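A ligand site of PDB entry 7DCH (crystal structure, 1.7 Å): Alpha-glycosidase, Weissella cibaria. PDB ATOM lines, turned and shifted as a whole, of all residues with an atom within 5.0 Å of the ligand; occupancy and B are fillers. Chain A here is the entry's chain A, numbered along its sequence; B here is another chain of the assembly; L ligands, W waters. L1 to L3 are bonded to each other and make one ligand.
His 214 touches the ligand. CD1 of Tyr 216 touches O5 of LG2 L2 (3.3 Å). Phe 306 touches the ligand. CE of Met 312 touches O3 of LG3 L3, at 3.5 Å. CG2 of Val 346 touches O3 of LIG L1 (3.2 Å). NE1 of Trp 376 touches O1 of LIG L1, 3.6 Å away. OH of Tyr 46 of chain B touches C2 of LIG L1 (3.6 Å). Hydrophobic or aromatic side chains within 4 Å of the ligand: His 214, Tyr 216, His 256, Phe 306, Met 312, Val 346, Trp 376 and His 439. Within 4 Å of the ligand: His 214, Tyr 216, His 256, Glu 296, Phe 306, Met 312, Arg 343, Asp 345, Val 346, Gln 374, Trp 376, His 439, Asp 440, Asp 484, Arg 488, Tyr 46 of chain B and Arg 49 of chain B.
Water W1 bridges O1 of LIG L1 and ND2 of Asn 120 of chain B. Water W3 lies within hydrogen-bond range of O2 of LIG L1, OD1 of Asn 348 and O of Gln 374. Water W5 lies within hydrogen-bond range of an oxygen (O2) of LIG L1 (2.7 Å), the side-chain carboxylate (OE2) of Glu 349 (2.8 Å), the side-chain amide nitrogen (ND2) of Asn 348 (3.0 Å) and the side-chain hydroxyl (OH) of Tyr 46 of chain B (3.3 Å). Water W7 lies within hydrogen-bond range of the side-chain carboxylate (OD2) of Asp 440 (2.7 Å), the indole nitrogen (NE1) of Trp 376 (3.1 Å), the side-chain amide nitrogen (NE2) of Gln 374 (3.1 Å) and an oxygen (O4) of LIG L1 (3.3 Å). Water W2 bridges OD2 of Asp 484 and OD1 of Asp 440. Water W6 lies within hydrogen-bond range of N of Trp 376 (2.8 Å), ND2 of Asn 348 (3.3 Å) and O2 of LIG L1 (3.4 Å).
OD2 of Asp 440 is in hydrogen-bond range of O1 of LG2 L2 (2.5 Å). OD2 of Asp 484 sits at hydrogen-bond distance from O2 of LG3 L3 (2.7 Å). OE1 of Gln 374 sits at hydrogen-bond distance from O3 of LIG L1, 2.7 Å away. An oxygen (O5) of LG2 L2 sits at hydrogen-bond distance from the side-chain carboxylate (OD2) of Asp 345 (2.8 Å). NH2 of Arg 488 sits at hydrogen-bond distance from O1 of LG3 L3, 2.9 Å away. An oxygen (O5) of LG2 L2 is in hydrogen-bond range of a ring nitrogen (NE2) of His 256 (3.0 Å). An oxygen (O1) of LG2 L2 is in hydrogen-bond range of the guanidinium group (NH2) of Arg 343 (3.0 Å). A ring nitrogen (NE2) of His 439 is in hydrogen-bond range of an oxygen (O2) of LG2 L2 (3.1 Å). The guanidinium group of Arg 49 of chain B is in hydrogen-bond range of an oxygen (O5) of LIG L1 (3.3 Å). The side-chain carboxylate of Glu 296 lies within salt-bridge range of a nitrogen (N1) of LG3 L3 (3.9 Å).
The side-chain carboxylate of Asp 440 lies within salt-bridge range of the guanidinium group of Arg 488 (3.5 Å). OE1 of Gln 374 sits at hydrogen-bond distance from N of Val 346, at 3.1 Å. NH1 of Arg 343 lies within salt-bridge range of OD1 of Asp 345 (2.9 Å). A ring nitrogen (NE2) of His 256 sits at hydrogen-bond distance from the side-chain sulfur (SD) of Met 312, at 3.8 Å. The side-chain hydroxyl (OH) of Tyr 216 sits at hydrogen-bond distance from a ring nitrogen (NE2) of His 439, 3.1 Å away. The backbone NH (N) of Glu 296 sits at hydrogen-bond distance from the side-chain amide oxygen (OD1) of Asn 294. A ring nitrogen (ND1) of His 214 is in hydrogen-bond range of the backbone NH (N) of Tyr 216, at 3.0 Å. OH of Tyr 46 of chain B lies within hydrogen-bond range of OE2 of Glu 349 (2.6 Å).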
ATOM      1  N   ARG A 176      -5.075 -12.591  18.348  1.00  0.00           N
ATOM      2  CA  ARG A 176      -6.237 -11.713  18.259  1.00  0.00           C
ATOM      3  C   ARG A 176      -6.644 -11.173  19.620  1.00  0.00           C
ATOM      4  O   ARG A 176      -7.182 -10.056  19.715  1.00  0.00           O
ATOM      5  CB  ARG A 176      -7.419 -12.449  17.621  1.00  0.00           C
ATOM      6  CG  ARG A 176      -7.188 -12.929  16.179  1.00  0.00           C
ATOM      7  CD  ARG A 176      -7.173 -14.470  16.065  1.00  0.00           C
ATOM      8  NE  ARG A 176      -5.898 -15.078  16.472  1.00  0.00           N
ATOM      9  CZ  ARG A 176      -5.744 -15.900  17.503  1.00  0.00           C
ATOM     10  NH1 ARG A 176      -6.795 -16.261  18.237  1.00  0.00           N
ATOM     11  NH2 ARG A 176      -4.553 -16.397  17.785  1.00  0.00           N
ATOM     12  N   HIS A 214      -8.756  -3.862  20.689  1.00  0.00           N
ATOM     13  CA  HIS A 214      -8.885  -2.838  19.661  1.00  0.00           C
ATOM     14  C   HIS A 214      -9.996  -1.817  19.957  1.00  0.00           C
ATOM     15  O   HIS A 214      -9.911  -0.682  19.477  1.00  0.00           O
ATOM     16  CB  HIS A 214      -9.167  -3.502  18.322  1.00  0.00           C
ATOM     17  CG  HIS A 214     -10.325  -4.432  18.356  1.00  0.00           C
ATOM     18  ND1 HIS A 214     -11.631  -3.994  18.289  1.00  0.00           N
ATOM     19  CD2 HIS A 214     -10.378  -5.787  18.407  1.00  0.00           C
ATOM     20  CE1 HIS A 214     -12.439  -5.044  18.333  1.00  0.00           C
ATOM     21  NE2 HIS A 214     -11.701  -6.138  18.387  1.00  0.00           N
ATOM     22  N   TYR A 216     -13.145  -1.518  19.159  1.00  0.00           N
ATOM     23  CA  TYR A 216     -14.217  -1.173  18.236  1.00  0.00           C
ATOM     24  C   TYR A 216     -15.552  -1.792  18.605  1.00  0.00           C
ATOM     25  O   TYR A 216     -16.551  -1.554  17.913  1.00  0.00           O
ATOM     26  CB  TYR A 216     -13.836  -1.576  16.802  1.00  0.00           C
ATOM     27  CG  TYR A 216     -12.832  -0.639  16.164  1.00  0.00           C
ATOM     28  CD1 TYR A 216     -13.271   0.467  15.435  1.00  0.00           C
ATOM     29  CD2 TYR A 216     -11.457  -0.882  16.255  1.00  0.00           C
ATOM     30  CE1 TYR A 216     -12.367   1.312  14.813  1.00  0.00           C
ATOM     31  CE2 TYR A 216     -10.548  -0.043  15.638  1.00  0.00           C
ATOM     32  CZ  TYR A 216     -11.009   1.055  14.926  1.00  0.00           C
ATOM     33  OH  TYR A 216     -10.113   1.895  14.328  1.00  0.00           O
ATOM     34  N   VAL A 253     -16.738   5.367  16.567  1.00  0.00           N
ATOM     35  CA  VAL A 253     -17.223   4.086  16.075  1.00  0.00           C
ATOM     36  C   VAL A 253     -18.728   4.116  16.213  1.00  0.00           C
ATOM     37  O   VAL A 253     -19.286   3.589  17.187  1.00  0.00           O
ATOM     38  CB  VAL A 253     -16.597   2.918  16.867  1.00  0.00           C
ATOM     39  CG1 VAL A 253     -16.931   1.565  16.251  1.00  0.00           C
ATOM     40  CG2 VAL A 253     -15.070   3.104  16.974  1.00  0.00           C
ATOM     41  N   HIS A 256     -21.824   0.791  14.735  1.00  0.00           N
ATOM     42  CA  HIS A 256     -22.246  -0.319  15.554  1.00  0.00           C
ATOM     43  C   HIS A 256     -21.738  -0.083  16.960  1.00  0.00           C
ATOM     44  O   HIS A 256     -20.845   0.737  17.194  1.00  0.00           O
ATOM     45  CB  HIS A 256     -21.694  -1.633  14.998  1.00  0.00           C
ATOM     46  CG  HIS A 256     -20.249  -1.546  14.582  1.00  0.00           C
ATOM     47  ND1 HIS A 256     -19.866  -1.222  13.292  1.00  0.00           N
ATOM     48  CD2 HIS A 256     -19.106  -1.754  15.287  1.00  0.00           C
ATOM     49  CE1 HIS A 256     -18.541  -1.211  13.229  1.00  0.00           C
ATOM     50  NE2 HIS A 256     -18.060  -1.564  14.418  1.00  0.00           N
ATOM     51  N   ASN A 294     -15.662 -19.622  15.153  1.00  0.00           N
ATOM     52  CA  ASN A 294     -15.027 -18.338  14.907  1.00  0.00           C
ATOM     53  C   ASN A 294     -15.819 -17.282  15.680  1.00  0.00           C
ATOM     54  O   ASN A 294     -16.986 -17.038  15.367  1.00  0.00           O
ATOM     55  CB  ASN A 294     -15.020 -18.039  13.407  1.00  0.00           C
ATOM     56  CG  ASN A 294     -14.392 -16.700  13.075  1.00  0.00           C
ATOM     57  OD1 ASN A 294     -14.046 -15.914  13.961  1.00  0.00           O
ATOM     58  ND2 ASN A 294     -14.235 -16.433  11.773  1.00  0.00           N
ATOM     59  N   GLU A 296     -15.825 -14.241  15.550  1.00  0.00           N
ATOM     60  CA  GLU A 296     -16.216 -13.096  14.730  1.00  0.00           C
ATOM     61  C   GLU A 296     -17.260 -13.425  13.657  1.00  0.00           C
ATOM     62  O   GLU A 296     -17.552 -12.563  12.821  1.00  0.00           O
ATOM     63  CB  GLU A 296     -14.982 -12.489  14.056  1.00  0.00           C
ATOM     64  CG  GLU A 296     -13.801 -12.242  14.963  1.00  0.00           C
ATOM     65  CD  GLU A 296     -13.959 -11.001  15.808  1.00  0.00           C
ATOM     66  OE1 GLU A 296     -15.102 -10.540  15.980  1.00  0.00           O
ATOM     67  OE2 GLU A 296     -12.930 -10.473  16.290  1.00  0.00           O
ATOM     68  N   PHE A 306     -22.126  -5.249  12.034  1.00  0.00           N
ATOM     69  CA  PHE A 306     -20.932  -5.079  11.230  1.00  0.00           C
ATOM     70  C   PHE A 306     -20.552  -6.434  10.637  1.00  0.00           C
ATOM     71  O   PHE A 306     -20.569  -7.442  11.348  1.00  0.00           O
ATOM     72  CB  PHE A 306     -19.751  -4.553  12.043  1.00  0.00           C
ATOM     73  CG  PHE A 306     -18.494  -4.494  11.237  1.00  0.00           C
ATOM     74  CD1 PHE A 306     -18.378  -3.567  10.211  1.00  0.00           C
ATOM     75  CD2 PHE A 306     -17.455  -5.385  11.466  1.00  0.00           C
ATOM     76  CE1 PHE A 306     -17.235  -3.501   9.430  1.00  0.00           C
ATOM     77  CE2 PHE A 306     -16.290  -5.340  10.669  1.00  0.00           C
ATOM     78  CZ  PHE A 306     -16.193  -4.373   9.638  1.00  0.00           C
ATOM     79  N   THR A 309     -20.343 -10.282  12.259  1.00  0.00           N
ATOM     80  CA  THR A 309     -19.978 -10.589  13.643  1.00  0.00           C
ATOM     81  C   THR A 309     -21.144 -10.288  14.576  1.00  0.00           C
ATOM     82  O   THR A 309     -21.604  -9.150  14.647  1.00  0.00           O
ATOM     83  CB  THR A 309     -18.746  -9.831  14.117  1.00  0.00           C
ATOM     84  OG1 THR A 309     -18.687  -9.987  15.546  1.00  0.00           O
ATOM     85  CG2 THR A 309     -18.793  -8.367  13.784  1.00  0.00           C
ATOM     86  N   MET A 312     -21.197  -7.086  17.269  1.00  0.00           N
ATOM     87  CA  MET A 312     -21.238  -5.692  16.826  1.00  0.00           C
ATOM     88  C   MET A 312     -22.568  -5.401  16.156  1.00  0.00           C
ATOM     89  O   MET A 312     -22.625  -5.118  14.955  1.00  0.00           O
ATOM     90  CB  MET A 312     -20.070  -5.389  15.879  1.00  0.00           C
ATOM     91  CG  MET A 312     -18.709  -5.456  16.574  1.00  0.00           C
ATOM     92  SD  MET A 312     -17.362  -5.112  15.435  1.00  0.00           S
ATOM     93  CE  MET A 312     -16.026  -4.889  16.634  1.00  0.00           C
ATOM     94  N   ARG A 343     -12.142  10.866  13.320  1.00  0.00           N
ATOM     95  CA  ARG A 343     -12.051   9.838  12.281  1.00  0.00           C
ATOM     96  C   ARG A 343     -13.265   8.927  12.438  1.00  0.00           C
ATOM     97  O   ARG A 343     -13.539   8.437  13.541  1.00  0.00           O
ATOM     98  CB  ARG A 343     -10.732   9.081  12.390  1.00  0.00           C
ATOM     99  CG  ARG A 343     -10.509   7.922  11.343  1.00  0.00           C
ATOM    100  CD  ARG A 343     -11.036   6.576  11.819  1.00  0.00           C
ATOM    101  NE  ARG A 343     -10.463   5.442  11.083  1.00  0.00           N
ATOM    102  CZ  ARG A 343     -10.913   4.190  11.159  1.00  0.00           C
ATOM    103  NH1 ARG A 343     -11.948   3.912  11.950  1.00  0.00           N
ATOM    104  NH2 ARG A 343     -10.332   3.221  10.457  1.00  0.00           N
ATOM    105  N   ASP A 345     -15.331   5.703  11.826  1.00  0.00           N
ATOM    106  CA  ASP A 345     -15.258   4.286  11.470  1.00  0.00           C
ATOM    107  C   ASP A 345     -16.447   3.846  10.617  1.00  0.00           C
ATOM    108  O   ASP A 345     -17.597   4.190  10.913  1.00  0.00           O
ATOM    109  CB  ASP A 345     -15.223   3.478  12.761  1.00  0.00           C
ATOM    110  CG  ASP A 345     -14.930   2.011  12.531  1.00  0.00           C
ATOM    111  OD1 ASP A 345     -13.876   1.724  11.915  1.00  0.00           O
ATOM    112  OD2 ASP A 345     -15.714   1.163  13.016  1.00  0.00           O
ATOM    113  N   VAL A 346     -16.173   3.026   9.586  1.00  0.00           N
ATOM    114  CA  VAL A 346     -17.202   2.501   8.666  1.00  0.00           C
ATOM    115  C   VAL A 346     -18.218   3.587   8.300  1.00  0.00           C
ATOM    116  O   VAL A 346     -19.437   3.371   8.322  1.00  0.00           O
ATOM    117  CB  VAL A 346     -17.922   1.281   9.271  1.00  0.00           C
ATOM    118  CG1 VAL A 346     -18.478   0.430   8.119  1.00  0.00           C
ATOM    119  CG2 VAL A 346     -17.005   0.460  10.153  1.00  0.00           C
ATOM    120  N   ASN A 348     -19.309   4.995   5.694  1.00  0.00           N
ATOM    121  CA  ASN A 348     -20.182   4.893   4.539  1.00  0.00           C
ATOM    122  C   ASN A 348     -21.475   4.159   4.860  1.00  0.00           C
ATOM    123  O   ASN A 348     -22.452   4.314   4.126  1.00  0.00           O
ATOM    124  CB  ASN A 348     -19.441   4.180   3.414  1.00  0.00           C
ATOM    125  CG  ASN A 348     -18.855   2.824   3.848  1.00  0.00           C
ATOM    126  OD1 ASN A 348     -18.632   2.532   5.020  1.00  0.00           O
ATOM    127  ND2 ASN A 348     -18.528   2.018   2.857  1.00  0.00           N
ATOM    128  N   GLU A 349     -21.517   3.408   5.959  1.00  0.00           N
ATOM    129  CA  GLU A 349     -22.690   2.607   6.269  1.00  0.00           C
ATOM    130  C   GLU A 349     -23.659   3.343   7.194  1.00  0.00           C
ATOM    131  O   GLU A 349     -24.670   2.755   7.607  1.00  0.00           O
ATOM    132  CB  GLU A 349     -22.239   1.231   6.825  1.00  0.00           C
ATOM    133  CG  GLU A 349     -21.505   0.430   5.735  1.00  0.00           C
ATOM    134  CD  GLU A 349     -21.003  -0.962   6.181  1.00  0.00           C
ATOM    135  OE1 GLU A 349     -21.477  -1.482   7.233  1.00  0.00           O
ATOM    136  OE2 GLU A 349     -20.139  -1.527   5.467  1.00  0.00           O
ATOM    137  N   GLN A 374     -13.791   7.056   7.158  1.00  0.00           N
ATOM    138  CA  GLN A 374     -13.071   5.863   6.737  1.00  0.00           C
ATOM    139  C   GLN A 374     -13.918   5.142   5.691  1.00  0.00           C
ATOM    140  O   GLN A 374     -14.857   4.419   6.034  1.00  0.00           O
ATOM    141  CB  GLN A 374     -12.754   4.927   7.895  1.00  0.00           C
ATOM    142  CG  GLN A 374     -11.854   3.751   7.443  1.00  0.00           C
ATOM    143  CD  GLN A 374     -12.201   2.445   8.119  1.00  0.00           C
ATOM    144  OE1 GLN A 374     -13.234   2.342   8.771  1.00  0.00           O
ATOM    145  NE2 GLN A 374     -11.354   1.437   7.962  1.00  0.00           N
ATOM    146  N   TRP A 376     -13.347   3.046   1.828  1.00  0.00           N
ATOM    147  CA  TRP A 376     -12.387   2.459   0.872  1.00  0.00           C
ATOM    148  C   TRP A 376     -12.708   2.766  -0.591  1.00  0.00           C
ATOM    149  O   TRP A 376     -11.809   2.684  -1.431  1.00  0.00           O
ATOM    150  CB  TRP A 376     -12.357   0.941   1.058  1.00  0.00           C
ATOM    151  CG  TRP A 376     -11.503   0.470   2.186  1.00  0.00           C
ATOM    152  CD1 TRP A 376     -11.821   0.449   3.510  1.00  0.00           C
ATOM    153  CD2 TRP A 376     -10.197  -0.108   2.070  1.00  0.00           C
ATOM    154  NE1 TRP A 376     -10.765  -0.104   4.235  1.00  0.00           N
ATOM    155  CE2 TRP A 376      -9.758  -0.437   3.371  1.00  0.00           C
ATOM    156  CE3 TRP A 376      -9.343  -0.363   0.992  1.00  0.00           C
ATOM    157  CZ2 TRP A 376      -8.515  -1.028   3.624  1.00  0.00           C
ATOM    158  CZ3 TRP A 376      -8.112  -0.941   1.237  1.00  0.00           C
ATOM    159  CH2 TRP A 376      -7.700  -1.261   2.540  1.00  0.00           C
ATOM    160  N   HIS A 439      -3.575  -0.264  11.058  1.00  0.00           N
ATOM    161  CA  HIS A 439      -3.883  -1.369  11.959  1.00  0.00           C
ATOM    162  C   HIS A 439      -4.706  -2.428  11.284  1.00  0.00           C
ATOM    163  O   HIS A 439      -5.040  -3.412  11.935  1.00  0.00           O
ATOM    164  CB  HIS A 439      -4.644  -0.850  13.175  1.00  0.00           C
ATOM    165  CG  HIS A 439      -5.930  -0.172  12.819  1.00  0.00           C
ATOM    166  ND1 HIS A 439      -5.993   0.912  11.972  1.00  0.00           N
ATOM    167  CD2 HIS A 439      -7.199  -0.444  13.175  1.00  0.00           C
ATOM    168  CE1 HIS A 439      -7.250   1.291  11.840  1.00  0.00           C
ATOM    169  NE2 HIS A 439      -8.005   0.485  12.570  1.00  0.00           N
ATOM    170  N   ASP A 440      -5.067  -2.219  10.015  1.00  0.00           N
ATOM    171  CA  ASP A 440      -5.875  -3.197   9.310  1.00  0.00           C
ATOM    172  C   ASP A 440      -5.108  -3.941   8.237  1.00  0.00           C
ATOM    173  O   ASP A 440      -5.479  -5.069   7.912  1.00  0.00           O
ATOM    174  CB  ASP A 440      -7.096  -2.525   8.663  1.00  0.00           C
ATOM    175  CG  ASP A 440      -8.138  -2.062   9.677  1.00  0.00           C
ATOM    176  OD1 ASP A 440      -8.296  -2.696  10.747  1.00  0.00           O
ATOM    177  OD2 ASP A 440      -8.802  -1.040   9.398  1.00  0.00           O
ATOM    178  N   ASP A 484      -3.590  -7.749  10.298  1.00  0.00           N
ATOM    179  CA  ASP A 484      -4.211  -7.840  11.623  1.00  0.00           C
ATOM    180  C   ASP A 484      -4.429  -9.294  12.026  1.00  0.00           C
ATOM    181  O   ASP A 484      -5.103 -10.030  11.283  1.00  0.00           O
ATOM    182  CB  ASP A 484      -5.532  -7.053  11.559  1.00  0.00           C
ATOM    183  CG  ASP A 484      -6.468  -7.301  12.729  1.00  0.00           C
ATOM    184  OD1 ASP A 484      -6.027  -7.749  13.808  1.00  0.00           O
ATOM    185  OD2 ASP A 484      -7.689  -7.043  12.573  1.00  0.00           O
ATOM    186  N   PRO A 485      -3.924  -9.756  13.198  1.00  0.00           N
ATOM    187  CA  PRO A 485      -3.315  -8.978  14.284  1.00  0.00           C
ATOM    188  C   PRO A 485      -1.818  -8.734  14.209  1.00  0.00           C
ATOM    189  O   PRO A 485      -1.245  -8.112  15.111  1.00  0.00           O
ATOM    190  CB  PRO A 485      -3.599  -9.844  15.527  1.00  0.00           C
ATOM    191  CG  PRO A 485      -3.544 -11.258  14.979  1.00  0.00           C
ATOM    192  CD  PRO A 485      -4.193 -11.155  13.594  1.00  0.00           C
ATOM    193  N   ARG A 488       0.015  -5.269  14.576  1.00  0.00           N
ATOM    194  CA  ARG A 488      -0.224  -4.579  15.832  1.00  0.00           C
ATOM    195  C   ARG A 488       0.804  -4.992  16.889  1.00  0.00           C
ATOM    196  O   ARG A 488       0.469  -5.141  18.067  1.00  0.00           O
ATOM    197  CB  ARG A 488      -1.644  -4.836  16.339  1.00  0.00           C
ATOM    198  CG  ARG A 488      -2.699  -4.258  15.407  1.00  0.00           C
ATOM    199  CD  ARG A 488      -4.055  -4.894  15.623  1.00  0.00           C
ATOM    200  NE  ARG A 488      -5.001  -4.396  14.609  1.00  0.00           N
ATOM    201  CZ  ARG A 488      -6.313  -4.548  14.692  1.00  0.00           C
ATOM    202  NH1 ARG A 488      -6.844  -5.165  15.763  1.00  0.00           N
ATOM    203  NH2 ARG A 488      -7.085  -4.055  13.732  1.00  0.00           N
ATOM    204  N   TYR B  46     -19.560  -8.100   2.056  1.00  0.00           N
ATOM    205  CA  TYR B  46     -18.899  -8.885   3.081  1.00  0.00           C
ATOM    206  C   TYR B  46     -19.052 -10.381   2.855  1.00  0.00           C
ATOM    207  O   TYR B  46     -18.309 -11.188   3.434  1.00  0.00           O
ATOM    208  CB  TYR B  46     -19.470  -8.500   4.448  1.00  0.00           C
ATOM    209  CG  TYR B  46     -19.149  -7.078   4.876  1.00  0.00           C
ATOM    210  CD1 TYR B  46     -17.977  -6.815   5.575  1.00  0.00           C
ATOM    211  CD2 TYR B  46     -20.002  -6.018   4.590  1.00  0.00           C
ATOM    212  CE1 TYR B  46     -17.640  -5.531   5.977  1.00  0.00           C
ATOM    213  CE2 TYR B  46     -19.691  -4.717   4.984  1.00  0.00           C
ATOM    214  CZ  TYR B  46     -18.520  -4.484   5.685  1.00  0.00           C
ATOM    215  OH  TYR B  46     -18.201  -3.215   6.110  1.00  0.00           O
ATOM    216  N   ARG B  49     -15.601 -12.554   1.607  1.00  0.00           N
ATOM    217  CA  ARG B  49     -14.621 -12.963   2.620  1.00  0.00           C
ATOM    218  C   ARG B  49     -15.261 -13.828   3.708  1.00  0.00           C
ATOM    219  O   ARG B  49     -14.652 -14.796   4.179  1.00  0.00           O
ATOM    220  CB  ARG B  49     -13.953 -11.712   3.249  1.00  0.00           C
ATOM    221  CG  ARG B  49     -14.793 -10.735   4.230  1.00  0.00           C
ATOM    222  CD  ARG B  49     -14.041  -9.361   4.515  1.00  0.00           C
ATOM    223  NE  ARG B  49     -14.516  -8.650   5.712  1.00  0.00           N
ATOM    224  CZ  ARG B  49     -14.070  -7.456   6.148  1.00  0.00           C
ATOM    225  NH1 ARG B  49     -13.135  -6.788   5.487  1.00  0.00           N
ATOM    226  NH2 ARG B  49     -14.588  -6.932   7.256  1.00  0.00           N
ATOM    227  N   MET B 119     -13.803  -6.945  -1.832  1.00  0.00           N
ATOM    228  CA  MET B 119     -14.999  -6.111  -1.832  1.00  0.00           C
ATOM    229  C   MET B 119     -14.674  -4.705  -2.288  1.00  0.00           C
ATOM    230  O   MET B 119     -15.544  -4.013  -2.829  1.00  0.00           O
ATOM    231  CB  MET B 119     -15.670  -6.089  -0.453  1.00  0.00           C
ATOM    232  CG  MET B 119     -14.751  -5.736   0.707  1.00  0.00           C
ATOM    233  SD  MET B 119     -15.615  -5.960   2.302  1.00  0.00           S
ATOM    234  CE  MET B 119     -16.415  -4.397   2.446  1.00  0.00           C
ATOM    235  N   ASN B 120     -13.421  -4.269  -2.118  1.00  0.00           N
ATOM    236  CA  ASN B 120     -13.098  -2.882  -2.448  1.00  0.00           C
ATOM    237  C   ASN B 120     -12.863  -2.663  -3.943  1.00  0.00           C
ATOM    238  O   ASN B 120     -12.657  -1.516  -4.365  1.00  0.00           O
ATOM    239  CB  ASN B 120     -11.886  -2.454  -1.622  1.00  0.00           C
ATOM    240  CG  ASN B 120     -12.204  -2.479  -0.130  1.00  0.00           C
ATOM    241  OD1 ASN B 120     -13.294  -2.112   0.254  1.00  0.00           O
ATOM    242  ND2 ASN B 120     -11.254  -2.924   0.693  1.00  0.00           N
HETATM  243  C1  LIG L   1     -14.360  -2.897   5.741  1.00  0.00           C
HETATM  244  C2  LIG L   1     -14.972  -1.651   6.408  1.00  0.00           C
HETATM  245  C3  LIG L   1     -14.012  -0.958   7.333  1.00  0.00           C
HETATM  246  C4  LIG L   1     -13.526  -1.911   8.379  1.00  0.00           C
HETATM  247  C5  LIG L   1     -12.873  -3.116   7.697  1.00  0.00           C
HETATM  248  C6  LIG L   1     -12.435  -4.137   8.684  1.00  0.00           C
HETATM  249  O1  LIG L   1     -13.314  -2.503   4.930  1.00  0.00           O
HETATM  250  O2  LIG L   1     -15.424  -0.717   5.398  1.00  0.00           O
HETATM  251  O3  LIG L   1     -14.694   0.183   7.913  1.00  0.00           O
HETATM  252  O4  LIG L   1     -12.478  -1.368   9.213  1.00  0.00           O
HETATM  253  O5  LIG L   1     -13.780  -3.822   6.750  1.00  0.00           O
HETATM  254  O6  LIG L   1     -11.745  -5.094   7.925  1.00  0.00           O
HETATM  255  C1  LG2 L   2     -12.868  -0.604  10.290  1.00  0.00           C
HETATM  256  C2  LG2 L   2     -11.709  -0.455  11.278  1.00  0.00           C
HETATM  257  C3  LG2 L   2     -11.363  -1.838  11.763  1.00  0.00           C
HETATM  258  C4  LG2 L   2     -12.473  -2.404  12.599  1.00  0.00           C
HETATM  259  C5  LG2 L   2     -13.777  -2.452  11.792  1.00  0.00           C
HETATM  260  C6  LG2 L   2     -14.985  -2.644  12.669  1.00  0.00           C
HETATM  261  O1  LG2 L   2     -10.621   0.205  10.608  1.00  0.00           O
HETATM  262  O2  LG2 L   2     -10.117  -1.796  12.527  1.00  0.00           O
HETATM  263  O3  LG2 L   2     -12.109  -3.732  12.945  1.00  0.00           O
HETATM  264  O4  LG2 L   2     -13.996  -1.213  10.998  1.00  0.00           O
HETATM  265  O5  LG2 L   2     -15.154  -1.550  13.552  1.00  0.00           O
HETATM  266  C1  LG3 L   3     -12.155  -4.020  14.315  1.00  0.00           C
HETATM  267  O1  LG3 L   3      -9.806  -3.665  14.493  1.00  0.00           O
HETATM  268  C2  LG3 L   3     -10.831  -4.640  14.729  1.00  0.00           C
HETATM  269  C3  LG3 L   3     -10.015 -10.754  10.984  1.00  0.00           C
HETATM  270  C4  LG3 L   3     -10.558  -5.898  13.975  1.00  0.00           C
HETATM  271  O2  LG3 L   3      -9.383  -6.519  14.602  1.00  0.00           O
HETATM  272  C5  LG3 L   3     -11.712  -6.832  14.131  1.00  0.00           C
HETATM  273  N1  LG3 L   3     -11.482  -8.178  13.501  1.00  0.00           N
HETATM  274  C6  LG3 L   3     -13.066  -6.190  13.721  1.00  0.00           C
HETATM  275  O3  LG3 L   3     -13.259  -4.950  14.521  1.00  0.00           O
HETATM  276  C7  LG3 L   3     -14.220  -7.093  14.011  1.00  0.00           C
HETATM  277  C8  LG3 L   3     -11.446  -8.321  12.059  1.00  0.00           C
HETATM  278  C9  LG3 L   3     -12.250  -9.771  11.708  1.00  0.00           C
HETATM  279  O4  LG3 L   3     -13.313  -9.910  12.695  1.00  0.00           O
HETATM  280  C10 LG3 L   3     -11.526 -10.881  11.754  1.00  0.00           C
HETATM  281  O5  LG3 L   3     -12.249 -12.001  11.146  1.00  0.00           O
HETATM  282  O6  LG3 L   3      -9.331 -11.959  11.055  1.00  0.00           O
HETATM  283  C11 LG3 L   3      -9.296  -9.750  11.669  1.00  0.00           C
HETATM  284  C12 LG3 L   3     -10.066  -8.352  11.642  1.00  0.00           C
HETATM  285  C13 LG3 L   3      -8.605 -10.203  12.967  1.00  0.00           C
HETATM  286  O7  LG3 L   3      -9.572 -10.281  13.987  1.00  0.00           O
HETATM  287  O   HOH W   1     -11.677  -4.076   3.626  1.00  0.00           O
HETATM  288  O   HOH W   2      -8.852  -5.466  10.527  1.00  0.00           O
HETATM  289  O   HOH W   3     -15.944   1.900   5.395  1.00  0.00           O
HETATM  290  O   HOH W   4     -14.710  -1.393   2.475  1.00  0.00           O
HETATM  291  O   HOH W   5     -17.797  -0.615   4.124  1.00  0.00           O
HETATM  292  O   HOH W   6     -15.327   1.322   2.696  1.00  0.00           O
HETATM  293  O   HOH W   7     -10.071  -1.263   7.016  1.00  0.00           O
